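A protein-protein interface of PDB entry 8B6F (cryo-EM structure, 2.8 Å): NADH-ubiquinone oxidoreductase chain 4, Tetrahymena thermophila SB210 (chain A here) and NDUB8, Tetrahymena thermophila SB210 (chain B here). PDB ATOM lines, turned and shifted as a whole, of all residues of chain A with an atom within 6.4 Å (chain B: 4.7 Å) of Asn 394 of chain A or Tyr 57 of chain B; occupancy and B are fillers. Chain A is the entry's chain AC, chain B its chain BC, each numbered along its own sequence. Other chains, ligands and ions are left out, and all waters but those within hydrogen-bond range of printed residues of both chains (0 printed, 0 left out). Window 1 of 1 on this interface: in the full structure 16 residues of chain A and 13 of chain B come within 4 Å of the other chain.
O of Tyr 57 of chain B lies within hydrogen-bond range of ND2 of Asn 394 of chain A (3.2 Å).
OD1 of Asp 58 of chain B lies close to OD1 of Asn 394 of chain A.
The side-chain amino group of Lys 458 of chain A lies within hydrogen-bond range of the side-chain sulfur of Met 56 of chain B (2.7 Å).
The side-chain sulfur of Met 56 of chain B sits at hydrogen-bond distance from the side-chain amide nitrogen of Asn 462 of chain A (3.1 Å).
The side-chain amide nitrogen (ND2) of Asn 462 of chain A is in hydrogen-bond range of the backbone carbonyl oxygen (O) of Tyr 57 of chain B (3.1 Å).
N of Met 467 of chain A is in hydrogen-bond range of OD1 of Asp 58 of chain B (3.4 Å).
OE1 of Gln 59 of chain B is in hydrogen-bond range of N of Lys 469 of chain A (3.1 Å).
The backbone carbonyl oxygen of Thr 328 of chain A sits at hydrogen-bond distance from the backbone NH of Leu 390 of chain A.
The side-chain amide nitrogen (ND2) of Asn 394 of chain A sits at hydrogen-bond distance from the backbone carbonyl oxygen (O) of Asn 462 of chain A (2.8 Å).
The side-chain amide nitrogen of Asn 394 of chain A sits at hydrogen-bond distance from the backbone carbonyl oxygen of Phe 465 of chain A, at 2.9 Å.
OD1 of Asn 394 of chain A sits at hydrogen-bond distance from N of Met 467 of chain A (3.1 Å).
OG1 of Thr 52 of chain B touches CG2 of Thr 328 of chain A, at 3.3 Å.
CG2 of Thr 328 of chain A touches OD1 of Asn 53 of chain B, at 3.5 Å.
CG1 of Val 391 of chain A touches CD2 of Leu 47 of chain B, 3.9 Å away.
Tyr 57 of chain B touches Val 391 of chain A (CE1 to CG1, 3.8 Å).
Gln 59 of chain B touches Glu 392 of chain A.
Asn 394 of chain A touches Gln 59 of chain B.
Lys 458 of chain A touches Asn 53 of chain B.
Trp 55 of chain B touches Lys 458 of chain A (O to NZ, 3.9 Å).
CB of Gln 59 of chain B touches O of Met 467 of chain A, 3.5 Å away.
Gln 59 of chain B touches Pro 468 of chain A (OE1 to CA, 3.4 Å).
Of the printed residues of chain B, Lys 458 of chain A touches Asn 53, Trp 55 and Met 56.
Of the printed residues of chain B, Asn 462 of chain A touches Met 56 and Tyr 57.
Of the printed residues of chain A, Tyr 57 of chain B touches Val 391 (3.8 Å), Asn 394 (3.2 Å) and Asn 462 (3.1 Å).
The nearest printed residue of chain B that does not touch Asn 394 of chain A is Met 56 of chain B (6.4 Å).
The nearest printed residue of chain A that does not touch Tyr 57 of chain B is Leu 390 of chain A (4.004 Å).
The nearest printed residue of chain B that does not touch Met 467 of chain A is Tyr 57 of chain B (6.7 Å).
Hydrophobic or aromatic side chains of chain A that line the printed part of chain B: Leu 390 and Val 391.
Printed residues of chain B that touch a printed residue of chain A: Leu 47, Thr 52, Asn 53, Trp 55, Met 56, Tyr 57, Asp 58 and Gln 59.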
ATOM      1  N   THR A 328     -20.269 -17.693   2.066  1.00  0.00           N
ATOM      2  CA  THR A 328     -19.955 -16.288   1.848  1.00  0.00           C
ATOM      3  C   THR A 328     -18.616 -16.088   1.154  1.00  0.00           C
ATOM      4  O   THR A 328     -18.317 -14.969   0.726  1.00  0.00           O
ATOM      5  CB  THR A 328     -19.941 -15.523   3.176  1.00  0.00           C
ATOM      6  OG1 THR A 328     -18.972 -16.107   4.057  1.00  0.00           O
ATOM      7  CG2 THR A 328     -21.313 -15.554   3.830  1.00  0.00           C
ATOM      8  N   TYR A 385      -9.528  -5.840  -4.456  1.00  0.00           N
ATOM      9  CA  TYR A 385     -10.045  -5.779  -3.095  1.00  0.00           C
ATOM     10  C   TYR A 385      -9.336  -6.858  -2.288  1.00  0.00           C
ATOM     11  O   TYR A 385      -9.411  -8.040  -2.632  1.00  0.00           O
ATOM     12  CB  TYR A 385     -11.559  -5.998  -3.061  1.00  0.00           C
ATOM     13  CG  TYR A 385     -12.366  -4.963  -3.812  1.00  0.00           C
ATOM     14  CD1 TYR A 385     -12.755  -3.780  -3.199  1.00  0.00           C
ATOM     15  CD2 TYR A 385     -12.760  -5.182  -5.125  1.00  0.00           C
ATOM     16  CE1 TYR A 385     -13.502  -2.838  -3.879  1.00  0.00           C
ATOM     17  CE2 TYR A 385     -13.506  -4.248  -5.812  1.00  0.00           C
ATOM     18  CZ  TYR A 385     -13.874  -3.077  -5.184  1.00  0.00           C
ATOM     19  OH  TYR A 385     -14.618  -2.143  -5.866  1.00  0.00           O
ATOM     20  N   SER A 389     -14.209 -12.387   0.645  1.00  0.00           N
ATOM     21  CA  SER A 389     -15.325 -12.728   1.512  1.00  0.00           C
ATOM     22  C   SER A 389     -16.463 -11.747   1.284  1.00  0.00           C
ATOM     23  O   SER A 389     -16.236 -10.544   1.121  1.00  0.00           O
ATOM     24  CB  SER A 389     -14.939 -12.704   2.985  1.00  0.00           C
ATOM     25  OG  SER A 389     -16.059 -13.071   3.771  1.00  0.00           O
ATOM     26  N   LEU A 390     -17.689 -12.268   1.282  1.00  0.00           N
ATOM     27  CA  LEU A 390     -18.845 -11.436   0.976  1.00  0.00           C
ATOM     28  C   LEU A 390     -19.064 -10.354   2.026  1.00  0.00           C
ATOM     29  O   LEU A 390     -19.541  -9.263   1.696  1.00  0.00           O
ATOM     30  CB  LEU A 390     -20.094 -12.307   0.848  1.00  0.00           C
ATOM     31  CG  LEU A 390     -21.366 -11.596   0.388  1.00  0.00           C
ATOM     32  CD1 LEU A 390     -21.170 -10.974  -0.983  1.00  0.00           C
ATOM     33  CD2 LEU A 390     -22.534 -12.560   0.378  1.00  0.00           C
ATOM     34  N   VAL A 391     -18.733 -10.631   3.289  1.00  0.00           N
ATOM     35  CA  VAL A 391     -18.963  -9.645   4.341  1.00  0.00           C
ATOM     36  C   VAL A 391     -18.041  -8.446   4.164  1.00  0.00           C
ATOM     37  O   VAL A 391     -18.435  -7.301   4.415  1.00  0.00           O
ATOM     38  CB  VAL A 391     -18.800 -10.291   5.730  1.00  0.00           C
ATOM     39  CG1 VAL A 391     -19.768 -11.446   5.893  1.00  0.00           C
ATOM     40  CG2 VAL A 391     -17.371 -10.763   5.950  1.00  0.00           C
ATOM     41  N   GLU A 392     -16.802  -8.681   3.736  1.00  0.00           N
ATOM     42  CA  GLU A 392     -15.829  -7.610   3.559  1.00  0.00           C
ATOM     43  C   GLU A 392     -15.896  -6.952   2.187  1.00  0.00           C
ATOM     44  O   GLU A 392     -15.324  -5.871   2.013  1.00  0.00           O
ATOM     45  CB  GLU A 392     -14.413  -8.143   3.784  1.00  0.00           C
ATOM     46  CG  GLU A 392     -14.106  -8.537   5.216  1.00  0.00           C
ATOM     47  CD  GLU A 392     -12.679  -9.014   5.389  1.00  0.00           C
ATOM     48  OE1 GLU A 392     -12.102  -9.528   4.410  1.00  0.00           O
ATOM     49  OE2 GLU A 392     -12.129  -8.869   6.500  1.00  0.00           O
ATOM     50  N   VAL A 393     -16.571  -7.563   1.216  1.00  0.00           N
ATOM     51  CA  VAL A 393     -16.637  -7.058  -0.152  1.00  0.00           C
ATOM     52  C   VAL A 393     -18.090  -6.773  -0.489  1.00  0.00           C
ATOM     53  O   VAL A 393     -18.957  -7.632  -0.299  1.00  0.00           O
ATOM     54  CB  VAL A 393     -16.048  -8.057  -1.163  1.00  0.00           C
ATOM     55  CG1 VAL A 393     -16.071  -7.473  -2.563  1.00  0.00           C
ATOM     56  CG2 VAL A 393     -14.648  -8.424  -0.787  1.00  0.00           C
ATOM     57  N   ASN A 394     -18.352  -5.574  -1.000  1.00  0.00           N
ATOM     58  CA  ASN A 394     -19.709  -5.184  -1.342  1.00  0.00           C
ATOM     59  C   ASN A 394     -19.652  -4.015  -2.313  1.00  0.00           C
ATOM     60  O   ASN A 394     -18.748  -3.178  -2.243  1.00  0.00           O
ATOM     61  CB  ASN A 394     -20.503  -4.817  -0.083  1.00  0.00           C
ATOM     62  CG  ASN A 394     -21.929  -4.427  -0.388  1.00  0.00           C
ATOM     63  OD1 ASN A 394     -22.294  -3.256  -0.312  1.00  0.00           O
ATOM     64  ND2 ASN A 394     -22.746  -5.411  -0.745  1.00  0.00           N
ATOM     65  N   GLY A 395     -20.621  -3.970  -3.220  1.00  0.00           N
ATOM     66  CA  GLY A 395     -20.711  -2.873  -4.171  1.00  0.00           C
ATOM     67  C   GLY A 395     -19.573  -2.803  -5.165  1.00  0.00           C
ATOM     68  O   GLY A 395     -19.066  -1.709  -5.443  1.00  0.00           O
ATOM     69  N   ILE A 396     -19.165  -3.943  -5.723  1.00  0.00           N
ATOM     70  CA  ILE A 396     -18.042  -3.956  -6.658  1.00  0.00           C
ATOM     71  C   ILE A 396     -18.372  -3.147  -7.906  1.00  0.00           C
ATOM     72  O   ILE A 396     -17.506  -2.473  -8.473  1.00  0.00           O
ATOM     73  CB  ILE A 396     -17.664  -5.407  -7.010  1.00  0.00           C
ATOM     74  CG1 ILE A 396     -17.171  -6.143  -5.761  1.00  0.00           C
ATOM     75  CG2 ILE A 396     -16.605  -5.435  -8.106  1.00  0.00           C
ATOM     76  CD1 ILE A 396     -16.900  -7.620  -5.982  1.00  0.00           C
ATOM     77  N   LEU A 397     -19.626  -3.203  -8.354  1.00  0.00           N
ATOM     78  CA  LEU A 397     -19.981  -2.601  -9.635  1.00  0.00           C
ATOM     79  C   LEU A 397     -19.783  -1.092  -9.630  1.00  0.00           C
ATOM     80  O   LEU A 397     -19.408  -0.516 -10.656  1.00  0.00           O
ATOM     81  CB  LEU A 397     -21.430  -2.952  -9.987  1.00  0.00           C
ATOM     82  CG  LEU A 397     -21.931  -2.669 -11.411  1.00  0.00           C
ATOM     83  CD1 LEU A 397     -23.179  -3.476 -11.681  1.00  0.00           C
ATOM     84  CD2 LEU A 397     -22.237  -1.197 -11.659  1.00  0.00           C
ATOM     85  N   LYS A 458     -27.021 -15.590  -5.007  1.00  0.00           N
ATOM     86  CA  LYS A 458     -27.181 -14.698  -3.864  1.00  0.00           C
ATOM     87  C   LYS A 458     -25.868 -13.998  -3.530  1.00  0.00           C
ATOM     88  O   LYS A 458     -25.814 -12.768  -3.438  1.00  0.00           O
ATOM     89  CB  LYS A 458     -27.706 -15.491  -2.664  1.00  0.00           C
ATOM     90  CG  LYS A 458     -27.371 -14.913  -1.292  1.00  0.00           C
ATOM     91  CD  LYS A 458     -27.929 -13.513  -1.100  1.00  0.00           C
ATOM     92  CE  LYS A 458     -27.423 -12.913   0.201  1.00  0.00           C
ATOM     93  NZ  LYS A 458     -27.818 -11.490   0.347  1.00  0.00           N
ATOM     94  N   PHE A 461     -24.556 -11.631  -6.474  1.00  0.00           N
ATOM     95  CA  PHE A 461     -25.340 -10.405  -6.579  1.00  0.00           C
ATOM     96  C   PHE A 461     -25.085  -9.482  -5.396  1.00  0.00           C
ATOM     97  O   PHE A 461     -24.971  -8.264  -5.564  1.00  0.00           O
ATOM     98  CB  PHE A 461     -26.832 -10.734  -6.678  1.00  0.00           C
ATOM     99  CG  PHE A 461     -27.269 -11.208  -8.039  1.00  0.00           C
ATOM    100  CD1 PHE A 461     -26.749 -10.644  -9.193  1.00  0.00           C
ATOM    101  CD2 PHE A 461     -28.212 -12.212  -8.161  1.00  0.00           C
ATOM    102  CE1 PHE A 461     -27.156 -11.077 -10.438  1.00  0.00           C
ATOM    103  CE2 PHE A 461     -28.621 -12.651  -9.405  1.00  0.00           C
ATOM    104  CZ  PHE A 461     -28.092 -12.082 -10.544  1.00  0.00           C
ATOM    105  N   ASN A 462     -24.994 -10.040  -4.188  1.00  0.00           N
ATOM    106  CA  ASN A 462     -24.738  -9.204  -3.023  1.00  0.00           C
ATOM    107  C   ASN A 462     -23.379  -8.527  -3.126  1.00  0.00           C
ATOM    108  O   ASN A 462     -23.226  -7.362  -2.744  1.00  0.00           O
ATOM    109  CB  ASN A 462     -24.830 -10.038  -1.746  1.00  0.00           C
ATOM    110  CG  ASN A 462     -24.627  -9.207  -0.498  1.00  0.00           C
ATOM    111  OD1 ASN A 462     -23.516  -9.093   0.013  1.00  0.00           O
ATOM    112  ND2 ASN A 462     -25.705  -8.611  -0.005  1.00  0.00           N
ATOM    113  N   ALA A 463     -22.374  -9.246  -3.630  1.00  0.00           N
ATOM    114  CA  ALA A 463     -21.059  -8.644  -3.816  1.00  0.00           C
ATOM    115  C   ALA A 463     -21.089  -7.575  -4.902  1.00  0.00           C
ATOM    116  O   ALA A 463     -20.514  -6.493  -4.733  1.00  0.00           O
ATOM    117  CB  ALA A 463     -20.034  -9.724  -4.159  1.00  0.00           C
ATOM    118  N   THR A 464     -21.754  -7.858  -6.023  1.00  0.00           N
ATOM    119  CA  THR A 464     -21.772  -6.910  -7.131  1.00  0.00           C
ATOM    120  C   THR A 464     -22.506  -5.630  -6.760  1.00  0.00           C
ATOM    121  O   THR A 464     -22.064  -4.532  -7.114  1.00  0.00           O
ATOM    122  CB  THR A 464     -22.419  -7.552  -8.359  1.00  0.00           C
ATOM    123  OG1 THR A 464     -21.686  -8.725  -8.731  1.00  0.00           O
ATOM    124  CG2 THR A 464     -22.434  -6.580  -9.531  1.00  0.00           C
ATOM    125  N   PHE A 465     -23.627  -5.748  -6.061  1.00  0.00           N
ATOM    126  CA  PHE A 465     -24.457  -4.602  -5.727  1.00  0.00           C
ATOM    127  C   PHE A 465     -24.219  -4.171  -4.285  1.00  0.00           C
ATOM    128  O   PHE A 465     -23.529  -4.836  -3.511  1.00  0.00           O
ATOM    129  CB  PHE A 465     -25.935  -4.930  -5.959  1.00  0.00           C
ATOM    130  CG  PHE A 465     -26.232  -5.389  -7.354  1.00  0.00           C
ATOM    131  CD1 PHE A 465     -26.129  -4.513  -8.419  1.00  0.00           C
ATOM    132  CD2 PHE A 465     -26.610  -6.696  -7.601  1.00  0.00           C
ATOM    133  CE1 PHE A 465     -26.398  -4.930  -9.706  1.00  0.00           C
ATOM    134  CE2 PHE A 465     -26.880  -7.121  -8.885  1.00  0.00           C
ATOM    135  CZ  PHE A 465     -26.773  -6.236  -9.939  1.00  0.00           C
ATOM    136  N   GLY A 466     -24.810  -3.035  -3.932  1.00  0.00           N
ATOM    137  CA  GLY A 466     -24.584  -2.431  -2.636  1.00  0.00           C
ATOM    138  C   GLY A 466     -23.931  -1.072  -2.770  1.00  0.00           C
ATOM    139  O   GLY A 466     -24.032  -0.434  -3.820  1.00  0.00           O
ATOM    140  N   MET A 467     -23.245  -0.623  -1.724  1.00  0.00           N
ATOM    141  CA  MET A 467     -22.646   0.704  -1.728  1.00  0.00           C
ATOM    142  C   MET A 467     -21.304   0.671  -1.003  1.00  0.00           C
ATOM    143  O   MET A 467     -21.274   0.570   0.229  1.00  0.00           O
ATOM    144  CB  MET A 467     -23.599   1.702  -1.074  1.00  0.00           C
ATOM    145  CG  MET A 467     -23.291   3.153  -1.369  1.00  0.00           C
ATOM    146  SD  MET A 467     -24.788   4.140  -1.548  1.00  0.00           S
ATOM    147  CE  MET A 467     -25.697   3.666  -0.082  1.00  0.00           C
ATOM    148  N   PRO A 468     -20.176   0.752  -1.721  1.00  0.00           N
ATOM    149  CA  PRO A 468     -18.857   0.621  -1.061  1.00  0.00           C
ATOM    150  C   PRO A 468     -18.406   1.890  -0.342  1.00  0.00           C
ATOM    151  O   PRO A 468     -17.615   2.694  -0.831  1.00  0.00           O
ATOM    152  CB  PRO A 468     -17.936   0.270  -2.230  1.00  0.00           C
ATOM    153  CG  PRO A 468     -18.549   0.958  -3.396  1.00  0.00           C
ATOM    154  CD  PRO A 468     -20.040   0.948  -3.176  1.00  0.00           C
ATOM    155  N   LYS A 469     -18.932   2.078   0.866  1.00  0.00           N
ATOM    156  CA  LYS A 469     -18.600   3.228   1.694  1.00  0.00           C
ATOM    157  C   LYS A 469     -17.358   3.010   2.548  1.00  0.00           C
ATOM    158  O   LYS A 469     -16.825   3.978   3.099  1.00  0.00           O
ATOM    159  CB  LYS A 469     -19.793   3.569   2.598  1.00  0.00           C
ATOM    160  CG  LYS A 469     -19.605   4.785   3.497  1.00  0.00           C
ATOM    161  CD  LYS A 469     -19.351   6.046   2.694  1.00  0.00           C
ATOM    162  CE  LYS A 469     -19.196   7.250   3.603  1.00  0.00           C
ATOM    163  NZ  LYS A 469     -19.116   8.512   2.821  1.00  0.00           N
ATOM    164  N   LEU B  47     -21.161 -11.518  13.578  1.00  0.00           N
ATOM    165  CA  LEU B  47     -21.865 -12.092  12.435  1.00  0.00           C
ATOM    166  C   LEU B  47     -21.849 -13.604  12.606  1.00  0.00           C
ATOM    167  O   LEU B  47     -20.881 -14.274  12.245  1.00  0.00           O
ATOM    168  CB  LEU B  47     -21.214 -11.667  11.123  1.00  0.00           C
ATOM    169  CG  LEU B  47     -21.189 -10.169  10.785  1.00  0.00           C
ATOM    170  CD1 LEU B  47     -20.158  -9.409  11.607  1.00  0.00           C
ATOM    171  CD2 LEU B  47     -20.938  -9.955   9.303  1.00  0.00           C
ATOM    172  N   ASP B  51     -26.174 -17.557  10.669  1.00  0.00           N
ATOM    173  CA  ASP B  51     -26.958 -16.633   9.858  1.00  0.00           C
ATOM    174  C   ASP B  51     -26.305 -16.362   8.508  1.00  0.00           C
ATOM    175  O   ASP B  51     -26.570 -15.325   7.893  1.00  0.00           O
ATOM    176  CB  ASP B  51     -27.170 -15.317  10.606  1.00  0.00           C
ATOM    177  CG  ASP B  51     -28.049 -15.473  11.825  1.00  0.00           C
ATOM    178  OD1 ASP B  51     -28.971 -16.313  11.787  1.00  0.00           O
ATOM    179  OD2 ASP B  51     -27.825 -14.753  12.818  1.00  0.00           O
ATOM    180  N   THR B  52     -25.452 -17.268   8.037  1.00  0.00           N
ATOM    181  CA  THR B  52     -24.748 -17.044   6.783  1.00  0.00           C
ATOM    182  C   THR B  52     -25.744 -16.841   5.648  1.00  0.00           C
ATOM    183  O   THR B  52     -26.678 -17.628   5.475  1.00  0.00           O
ATOM    184  CB  THR B  52     -23.818 -18.219   6.479  1.00  0.00           C
ATOM    185  OG1 THR B  52     -23.111 -17.975   5.256  1.00  0.00           O
ATOM    186  CG2 THR B  52     -24.600 -19.524   6.362  1.00  0.00           C
ATOM    187  N   ASN B  53     -25.548 -15.771   4.883  1.00  0.00           N
ATOM    188  CA  ASN B  53     -26.408 -15.398   3.765  1.00  0.00           C
ATOM    189  C   ASN B  53     -27.848 -15.134   4.188  1.00  0.00           C
ATOM    190  O   ASN B  53     -28.727 -15.012   3.328  1.00  0.00           O
ATOM    191  CB  ASN B  53     -26.378 -16.459   2.656  1.00  0.00           C
ATOM    192  CG  ASN B  53     -25.197 -16.292   1.721  1.00  0.00           C
ATOM    193  OD1 ASN B  53     -24.285 -15.513   1.988  1.00  0.00           O
ATOM    194  ND2 ASN B  53     -25.209 -17.028   0.618  1.00  0.00           N
ATOM    195  N   TRP B  55     -28.421 -12.399   5.989  1.00  0.00           N
ATOM    196  CA  TRP B  55     -28.403 -10.945   6.009  1.00  0.00           C
ATOM    197  C   TRP B  55     -27.918 -10.443   4.658  1.00  0.00           C
ATOM    198  O   TRP B  55     -26.905 -10.926   4.143  1.00  0.00           O
ATOM    199  CB  TRP B  55     -27.496 -10.416   7.121  1.00  0.00           C
ATOM    200  CG  TRP B  55     -28.007 -10.699   8.491  1.00  0.00           C
ATOM    201  CD1 TRP B  55     -27.801 -11.829   9.224  1.00  0.00           C
ATOM    202  CD2 TRP B  55     -28.811  -9.835   9.299  1.00  0.00           C
ATOM    203  NE1 TRP B  55     -28.431 -11.722  10.440  1.00  0.00           N
ATOM    204  CE2 TRP B  55     -29.058 -10.506  10.510  1.00  0.00           C
ATOM    205  CE3 TRP B  55     -29.348  -8.559   9.113  1.00  0.00           C
ATOM    206  CZ2 TRP B  55     -29.818  -9.946  11.531  1.00  0.00           C
ATOM    207  CZ3 TRP B  55     -30.101  -8.002  10.128  1.00  0.00           C
ATOM    208  CH2 TRP B  55     -30.330  -8.695  11.322  1.00  0.00           C
ATOM    209  N   MET B  56     -28.643  -9.489   4.081  1.00  0.00           N
ATOM    210  CA  MET B  56     -28.215  -8.843   2.842  1.00  0.00           C
ATOM    211  C   MET B  56     -27.114  -7.862   3.218  1.00  0.00           C
ATOM    212  O   MET B  56     -27.366  -6.708   3.563  1.00  0.00           O
ATOM    213  CB  MET B  56     -29.384  -8.155   2.150  1.00  0.00           C
ATOM    214  CG  MET B  56     -29.077  -7.691   0.737  1.00  0.00           C
ATOM    215  SD  MET B  56     -28.740  -9.045  -0.406  1.00  0.00           S
ATOM    216  CE  MET B  56     -30.369  -9.764  -0.585  1.00  0.00           C
ATOM    217  N   TYR B  57     -25.872  -8.334   3.155  1.00  0.00           N
ATOM    218  CA  TYR B  57     -24.753  -7.561   3.673  1.00  0.00           C
ATOM    219  C   TYR B  57     -24.571  -6.271   2.887  1.00  0.00           C
ATOM    220  O   TYR B  57     -24.681  -6.248   1.659  1.00  0.00           O
ATOM    221  CB  TYR B  57     -23.470  -8.392   3.618  1.00  0.00           C
ATOM    222  CG  TYR B  57     -23.552  -9.674   4.412  1.00  0.00           C
ATOM    223  CD1 TYR B  57     -23.370  -9.674   5.787  1.00  0.00           C
ATOM    224  CD2 TYR B  57     -23.805 -10.884   3.785  1.00  0.00           C
ATOM    225  CE1 TYR B  57     -23.445 -10.843   6.516  1.00  0.00           C
ATOM    226  CE2 TYR B  57     -23.881 -12.058   4.504  1.00  0.00           C
ATOM    227  CZ  TYR B  57     -23.699 -12.031   5.870  1.00  0.00           C
ATOM    228  OH  TYR B  57     -23.773 -13.198   6.592  1.00  0.00           O
ATOM    229  N   ASP B  58     -24.298  -5.189   3.610  1.00  0.00           N
ATOM    230  CA  ASP B  58     -24.031  -3.899   2.995  1.00  0.00           C
ATOM    231  C   ASP B  58     -23.154  -3.089   3.936  1.00  0.00           C
ATOM    232  O   ASP B  58     -23.095  -3.352   5.138  1.00  0.00           O
ATOM    233  CB  ASP B  58     -25.326  -3.144   2.683  1.00  0.00           C
ATOM    234  CG  ASP B  58     -25.093  -1.923   1.821  1.00  0.00           C
ATOM    235  OD1 ASP B  58     -23.943  -1.714   1.389  1.00  0.00           O
ATOM    236  OD2 ASP B  58     -26.059  -1.172   1.574  1.00  0.00           O
ATOM    237  N   GLN B  59     -22.467  -2.102   3.371  1.00  0.00           N
ATOM    238  CA  GLN B  59     -21.589  -1.233   4.140  1.00  0.00           C
ATOM    239  C   GLN B  59     -22.269   0.053   4.586  1.00  0.00           C
ATOM    240  O   GLN B  59     -21.646   0.848   5.296  1.00  0.00           O
ATOM    241  CB  GLN B  59     -20.339  -0.897   3.322  1.00  0.00           C
ATOM    242  CG  GLN B  59     -19.554  -2.122   2.889  1.00  0.00           C
ATOM    243  CD  GLN B  59     -18.323  -1.770   2.090  1.00  0.00           C
ATOM    244  OE1 GLN B  59     -17.959  -0.603   1.972  1.00  0.00           O
ATOM    245  NE2 GLN B  59     -17.673  -2.783   1.530  1.00  0.00           N
